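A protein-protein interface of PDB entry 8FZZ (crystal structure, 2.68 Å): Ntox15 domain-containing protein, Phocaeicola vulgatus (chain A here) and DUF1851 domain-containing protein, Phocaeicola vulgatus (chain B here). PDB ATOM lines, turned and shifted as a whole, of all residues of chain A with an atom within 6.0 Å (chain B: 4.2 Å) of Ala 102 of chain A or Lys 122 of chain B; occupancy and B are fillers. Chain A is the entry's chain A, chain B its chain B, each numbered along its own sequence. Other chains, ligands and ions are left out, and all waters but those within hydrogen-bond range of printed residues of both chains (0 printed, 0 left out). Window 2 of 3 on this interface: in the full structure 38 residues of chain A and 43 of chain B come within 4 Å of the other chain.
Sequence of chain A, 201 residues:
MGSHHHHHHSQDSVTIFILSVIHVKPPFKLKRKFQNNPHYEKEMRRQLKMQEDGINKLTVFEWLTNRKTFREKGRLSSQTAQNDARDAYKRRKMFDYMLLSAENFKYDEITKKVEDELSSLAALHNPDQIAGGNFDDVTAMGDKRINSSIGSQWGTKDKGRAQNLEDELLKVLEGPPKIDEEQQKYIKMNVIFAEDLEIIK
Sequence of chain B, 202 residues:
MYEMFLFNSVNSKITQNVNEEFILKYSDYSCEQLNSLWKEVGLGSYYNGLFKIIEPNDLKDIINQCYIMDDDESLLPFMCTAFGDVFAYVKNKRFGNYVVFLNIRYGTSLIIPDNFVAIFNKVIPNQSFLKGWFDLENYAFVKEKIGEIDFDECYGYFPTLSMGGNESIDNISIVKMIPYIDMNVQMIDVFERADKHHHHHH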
ATOM      1  N   MET A  98     -11.919  -8.218 -19.537  1.00  0.00           N
ATOM      2  CA  MET A  98     -11.509  -7.572 -20.780  1.00  0.00           C
ATOM      3  C   MET A  98     -10.861  -8.516 -21.781  1.00  0.00           C
ATOM      4  O   MET A  98     -11.213  -8.463 -22.952  1.00  0.00           O
ATOM      5  CB  MET A  98     -10.590  -6.375 -20.487  1.00  0.00           C
ATOM      6  CG  MET A  98     -11.308  -5.271 -19.705  1.00  0.00           C
ATOM      7  SD  MET A  98     -10.203  -3.749 -19.080  1.00  0.00           S
ATOM      8  CE  MET A  98      -9.506  -3.081 -20.789  1.00  0.00           C
ATOM      9  N   LEU A  99      -9.947  -9.390 -21.354  1.00  0.00           N
ATOM     10  CA  LEU A  99      -9.387 -10.339 -22.314  1.00  0.00           C
ATOM     11  C   LEU A  99     -10.439 -11.339 -22.769  1.00  0.00           C
ATOM     12  O   LEU A  99     -10.444 -11.748 -23.936  1.00  0.00           O
ATOM     13  CB  LEU A  99      -8.188 -11.078 -21.731  1.00  0.00           C
ATOM     14  CG  LEU A  99      -7.131 -10.329 -20.927  1.00  0.00           C
ATOM     15  CD1 LEU A  99      -6.463 -11.273 -19.942  1.00  0.00           C
ATOM     16  CD2 LEU A  99      -6.114  -9.744 -21.868  1.00  0.00           C
ATOM     17  N   LEU A 100     -11.341 -11.733 -21.861  1.00  0.00           N
ATOM     18  CA  LEU A 100     -12.392 -12.692 -22.188  1.00  0.00           C
ATOM     19  C   LEU A 100     -13.255 -12.196 -23.342  1.00  0.00           C
ATOM     20  O   LEU A 100     -13.319 -12.827 -24.405  1.00  0.00           O
ATOM     21  CB  LEU A 100     -13.251 -12.966 -20.951  1.00  0.00           C
ATOM     22  CG  LEU A 100     -12.914 -14.227 -20.147  1.00  0.00           C
ATOM     23  CD1 LEU A 100     -14.105 -14.699 -19.291  1.00  0.00           C
ATOM     24  CD2 LEU A 100     -12.415 -15.335 -21.076  1.00  0.00           C
ATOM     25  N   SER A 101     -13.946 -11.074 -23.143  1.00  0.00           N
ATOM     26  CA  SER A 101     -14.769 -10.497 -24.197  1.00  0.00           C
ATOM     27  C   SER A 101     -13.892  -9.882 -25.291  1.00  0.00           C
ATOM     28  O   SER A 101     -12.715  -9.573 -25.084  1.00  0.00           O
ATOM     29  CB  SER A 101     -15.720  -9.445 -23.613  1.00  0.00           C
ATOM     30  OG  SER A 101     -16.073  -8.473 -24.584  1.00  0.00           O
ATOM     31  N   ALA A 102     -14.478  -9.727 -26.480  1.00  0.00           N
ATOM     32  CA  ALA A 102     -13.821  -9.046 -27.593  1.00  0.00           C
ATOM     33  C   ALA A 102     -14.455  -7.703 -27.914  1.00  0.00           C
ATOM     34  O   ALA A 102     -13.999  -7.022 -28.839  1.00  0.00           O
ATOM     35  CB  ALA A 102     -13.821  -9.925 -28.848  1.00  0.00           C
ATOM     36  N   GLU A 103     -15.494  -7.307 -27.182  1.00  0.00           N
ATOM     37  CA  GLU A 103     -16.103  -5.993 -27.310  1.00  0.00           C
ATOM     38  C   GLU A 103     -15.727  -5.167 -26.086  1.00  0.00           C
ATOM     39  O   GLU A 103     -15.923  -5.611 -24.948  1.00  0.00           O
ATOM     40  CB  GLU A 103     -17.625  -6.106 -27.459  1.00  0.00           C
ATOM     41  CG  GLU A 103     -18.237  -5.086 -28.429  1.00  0.00           C
ATOM     42  CD  GLU A 103     -17.745  -5.256 -29.870  1.00  0.00           C
ATOM     43  OE1 GLU A 103     -18.128  -6.255 -30.520  1.00  0.00           O
ATOM     44  OE2 GLU A 103     -16.979  -4.387 -30.351  1.00  0.00           O
ATOM     45  N   ASN A 104     -15.191  -3.971 -26.322  1.00  0.00           N
ATOM     46  CA  ASN A 104     -14.528  -3.209 -25.275  1.00  0.00           C
ATOM     47  C   ASN A 104     -15.511  -2.789 -24.185  1.00  0.00           C
ATOM     48  O   ASN A 104     -16.725  -2.716 -24.387  1.00  0.00           O
ATOM     49  CB  ASN A 104     -13.832  -1.979 -25.865  1.00  0.00           C
ATOM     50  CG  ASN A 104     -12.938  -2.326 -27.055  1.00  0.00           C
ATOM     51  OD1 ASN A 104     -12.508  -3.471 -27.222  1.00  0.00           O
ATOM     52  ND2 ASN A 104     -12.664  -1.334 -27.892  1.00  0.00           N
ATOM     53  N   VAL B 117      -0.174  -8.089 -22.085  1.00  0.00           N
ATOM     54  CA  VAL B 117      -1.183  -8.354 -23.103  1.00  0.00           C
ATOM     55  C   VAL B 117      -2.429  -7.516 -22.840  1.00  0.00           C
ATOM     56  O   VAL B 117      -2.923  -6.818 -23.731  1.00  0.00           O
ATOM     57  CB  VAL B 117      -1.498  -9.861 -23.162  1.00  0.00           C
ATOM     58  CG1 VAL B 117      -2.586 -10.146 -24.160  1.00  0.00           C
ATOM     59  CG2 VAL B 117      -0.247 -10.631 -23.520  1.00  0.00           C
ATOM     60  N   ALA B 118      -2.947  -7.551 -21.611  1.00  0.00           N
ATOM     61  CA  ALA B 118      -4.106  -6.713 -21.303  1.00  0.00           C
ATOM     62  C   ALA B 118      -3.777  -5.231 -21.464  1.00  0.00           C
ATOM     63  O   ALA B 118      -4.554  -4.476 -22.066  1.00  0.00           O
ATOM     64  CB  ALA B 118      -4.606  -6.999 -19.891  1.00  0.00           C
ATOM     65  N   PHE B 120      -1.414  -3.569 -23.292  1.00  0.00           N
ATOM     66  CA  PHE B 120      -1.157  -3.081 -24.645  1.00  0.00           C
ATOM     67  C   PHE B 120      -2.295  -3.386 -25.612  1.00  0.00           C
ATOM     68  O   PHE B 120      -2.490  -2.646 -26.584  1.00  0.00           O
ATOM     69  CB  PHE B 120       0.139  -3.684 -25.186  1.00  0.00           C
ATOM     70  CG  PHE B 120       1.374  -2.931 -24.781  1.00  0.00           C
ATOM     71  CD1 PHE B 120       1.781  -2.900 -23.458  1.00  0.00           C
ATOM     72  CD2 PHE B 120       2.126  -2.247 -25.723  1.00  0.00           C
ATOM     73  CE1 PHE B 120       2.917  -2.205 -23.084  1.00  0.00           C
ATOM     74  CE2 PHE B 120       3.261  -1.550 -25.353  1.00  0.00           C
ATOM     75  CZ  PHE B 120       3.656  -1.531 -24.033  1.00  0.00           C
ATOM     76  N   ASN B 121      -3.058  -4.451 -25.376  1.00  0.00           N
ATOM     77  CA  ASN B 121      -4.069  -4.846 -26.344  1.00  0.00           C
ATOM     78  C   ASN B 121      -5.462  -4.361 -25.999  1.00  0.00           C
ATOM     79  O   ASN B 121      -6.259  -4.137 -26.905  1.00  0.00           O
ATOM     80  CB  ASN B 121      -4.095  -6.364 -26.508  1.00  0.00           C
ATOM     81  CG  ASN B 121      -2.907  -6.877 -27.272  1.00  0.00           C
ATOM     82  OD1 ASN B 121      -2.343  -6.170 -28.094  1.00  0.00           O
ATOM     83  ND2 ASN B 121      -2.512  -8.109 -26.999  1.00  0.00           N
ATOM     84  N   LYS B 122      -5.791  -4.176 -24.734  1.00  0.00           N
ATOM     85  CA  LYS B 122      -7.155  -3.806 -24.417  1.00  0.00           C
ATOM     86  C   LYS B 122      -7.302  -2.549 -23.567  1.00  0.00           C
ATOM     87  O   LYS B 122      -8.415  -2.014 -23.499  1.00  0.00           O
ATOM     88  CB  LYS B 122      -7.878  -4.982 -23.735  1.00  0.00           C
ATOM     89  CG  LYS B 122      -8.566  -5.935 -24.741  1.00  0.00           C
ATOM     90  CD  LYS B 122     -10.073  -6.111 -24.443  1.00  0.00           C
ATOM     91  CE  LYS B 122     -10.852  -6.799 -25.583  1.00  0.00           C
ATOM     92  NZ  LYS B 122     -11.362  -5.841 -26.619  1.00  0.00           N
ATOM     93  N   VAL B 123      -6.241  -2.043 -22.943  1.00  0.00           N
ATOM     94  CA  VAL B 123      -6.336  -0.809 -22.163  1.00  0.00           C
ATOM     95  C   VAL B 123      -5.942   0.402 -22.992  1.00  0.00           C
ATOM     96  O   VAL B 123      -6.635   1.421 -22.988  1.00  0.00           O
ATOM     97  CB  VAL B 123      -5.501  -0.897 -20.863  1.00  0.00           C
ATOM     98  CG1 VAL B 123      -5.424   0.473 -20.191  1.00  0.00           C
ATOM     99  CG2 VAL B 123      -6.120  -1.901 -19.901  1.00  0.00           C
ATOM    100  N   ILE B 124      -4.846   0.300 -23.732  1.00  0.00           N
ATOM    101  CA  ILE B 124      -4.369   1.409 -24.554  1.00  0.00           C
ATOM    102  C   ILE B 124      -5.334   1.717 -25.701  1.00  0.00           C
ATOM    103  O   ILE B 124      -5.658   2.895 -25.918  1.00  0.00           O
ATOM    104  CB  ILE B 124      -2.946   1.130 -25.066  1.00  0.00           C
ATOM    105  CG1 ILE B 124      -1.968   1.127 -23.882  1.00  0.00           C
ATOM    106  CG2 ILE B 124      -2.554   2.137 -26.129  1.00  0.00           C
ATOM    107  CD1 ILE B 124      -0.515   1.267 -24.269  1.00  0.00           C
ATOM    108  N   PRO B 125      -5.845   0.725 -26.462  1.00  0.00           N
ATOM    109  CA  PRO B 125      -6.783   1.076 -27.539  1.00  0.00           C
ATOM    110  C   PRO B 125      -8.205   1.312 -27.041  1.00  0.00           C
ATOM    111  O   PRO B 125      -9.169   1.048 -27.768  1.00  0.00           O
ATOM    112  CB  PRO B 125      -6.713  -0.138 -28.484  1.00  0.00           C
ATOM    113  CG  PRO B 125      -5.563  -0.986 -27.988  1.00  0.00           C
ATOM    114  CD  PRO B 125      -5.488  -0.703 -26.522  1.00  0.00           C
ATOM    115  N   ASN B 126      -8.347   1.824 -25.817  1.00  0.00           N
ATOM    116  CA  ASN B 126      -9.645   2.044 -25.174  1.00  0.00           C
ATOM    117  C   ASN B 126      -9.642   3.464 -24.611  1.00  0.00           C
ATOM    118  O   ASN B 126      -9.060   3.712 -23.551  1.00  0.00           O
ATOM    119  CB  ASN B 126      -9.891   1.001 -24.080  1.00  0.00           C
ATOM    120  CG  ASN B 126     -11.286   1.081 -23.482  1.00  0.00           C
ATOM    121  OD1 ASN B 126     -11.686   2.119 -22.972  1.00  0.00           O
ATOM    122  ND2 ASN B 126     -12.026  -0.032 -23.525  1.00  0.00           N
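The side-chain hydroxyl (OG) of Ser 101 of chain A sits at hydrogen-bond distance from the backbone carbonyl oxygen (O) of Glu 103 of chain A, at 2.9 Å. O of Ala 118 of chain B is in hydrogen-bond range of N of Val 123 of chain B, 3.1 Å away.
Met 98 of chain A touches Lys 122 of chain B. CG2 of Val 123 of chain B touches CE of Met 98 of chain A (3.7 Å). CD2 of Leu 99 of chain A touches CA of Ala 118 of chain B (3.7 Å). Lys 122 of chain B touches Ser 101 of chain A (CE to O, 3.4 Å). Ala 102 of chain A touches Lys 122 of chain B. Asn 126 of chain B touches Asn 104 of chain A.
Ala 102 of chain A touches just one residue of chain B: Lys 122. Of the printed residues of chain B, Leu 99 of chain A touches Ala 118 (3.7 Å). Printed residues of chain B within 4 Å of Ser 101 of chain A: Lys 122. Printed residues of chain A within 4 Å of Ala 118 of chain B: Leu 99 (3.7 Å). The nearest printed residue of chain B that does not touch Leu 99 of chain A is Val 117 of chain B (4.2 Å).
Of the 7 printed residues of chain A, 5 touch a printed residue of chain B. Hydrophobic or aromatic side chains of chain A that line the printed part of chain B: Met 98 and Leu 99. Along chain A the printed residues that touch a printed residue of chain B span positions 98 to 104. Of the 9 printed residues of chain B, 4 touch a printed residue of chain A. Among the printed residues, no Asp or Glu carboxylate lies within 4 Å of a Lys or Arg side-chain nitrogen of the other chain.
OD1 of Asn 104 of chain A is in hydrogen-bond range of NZ of Lys 122 of chain B, 2.7 Å away.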
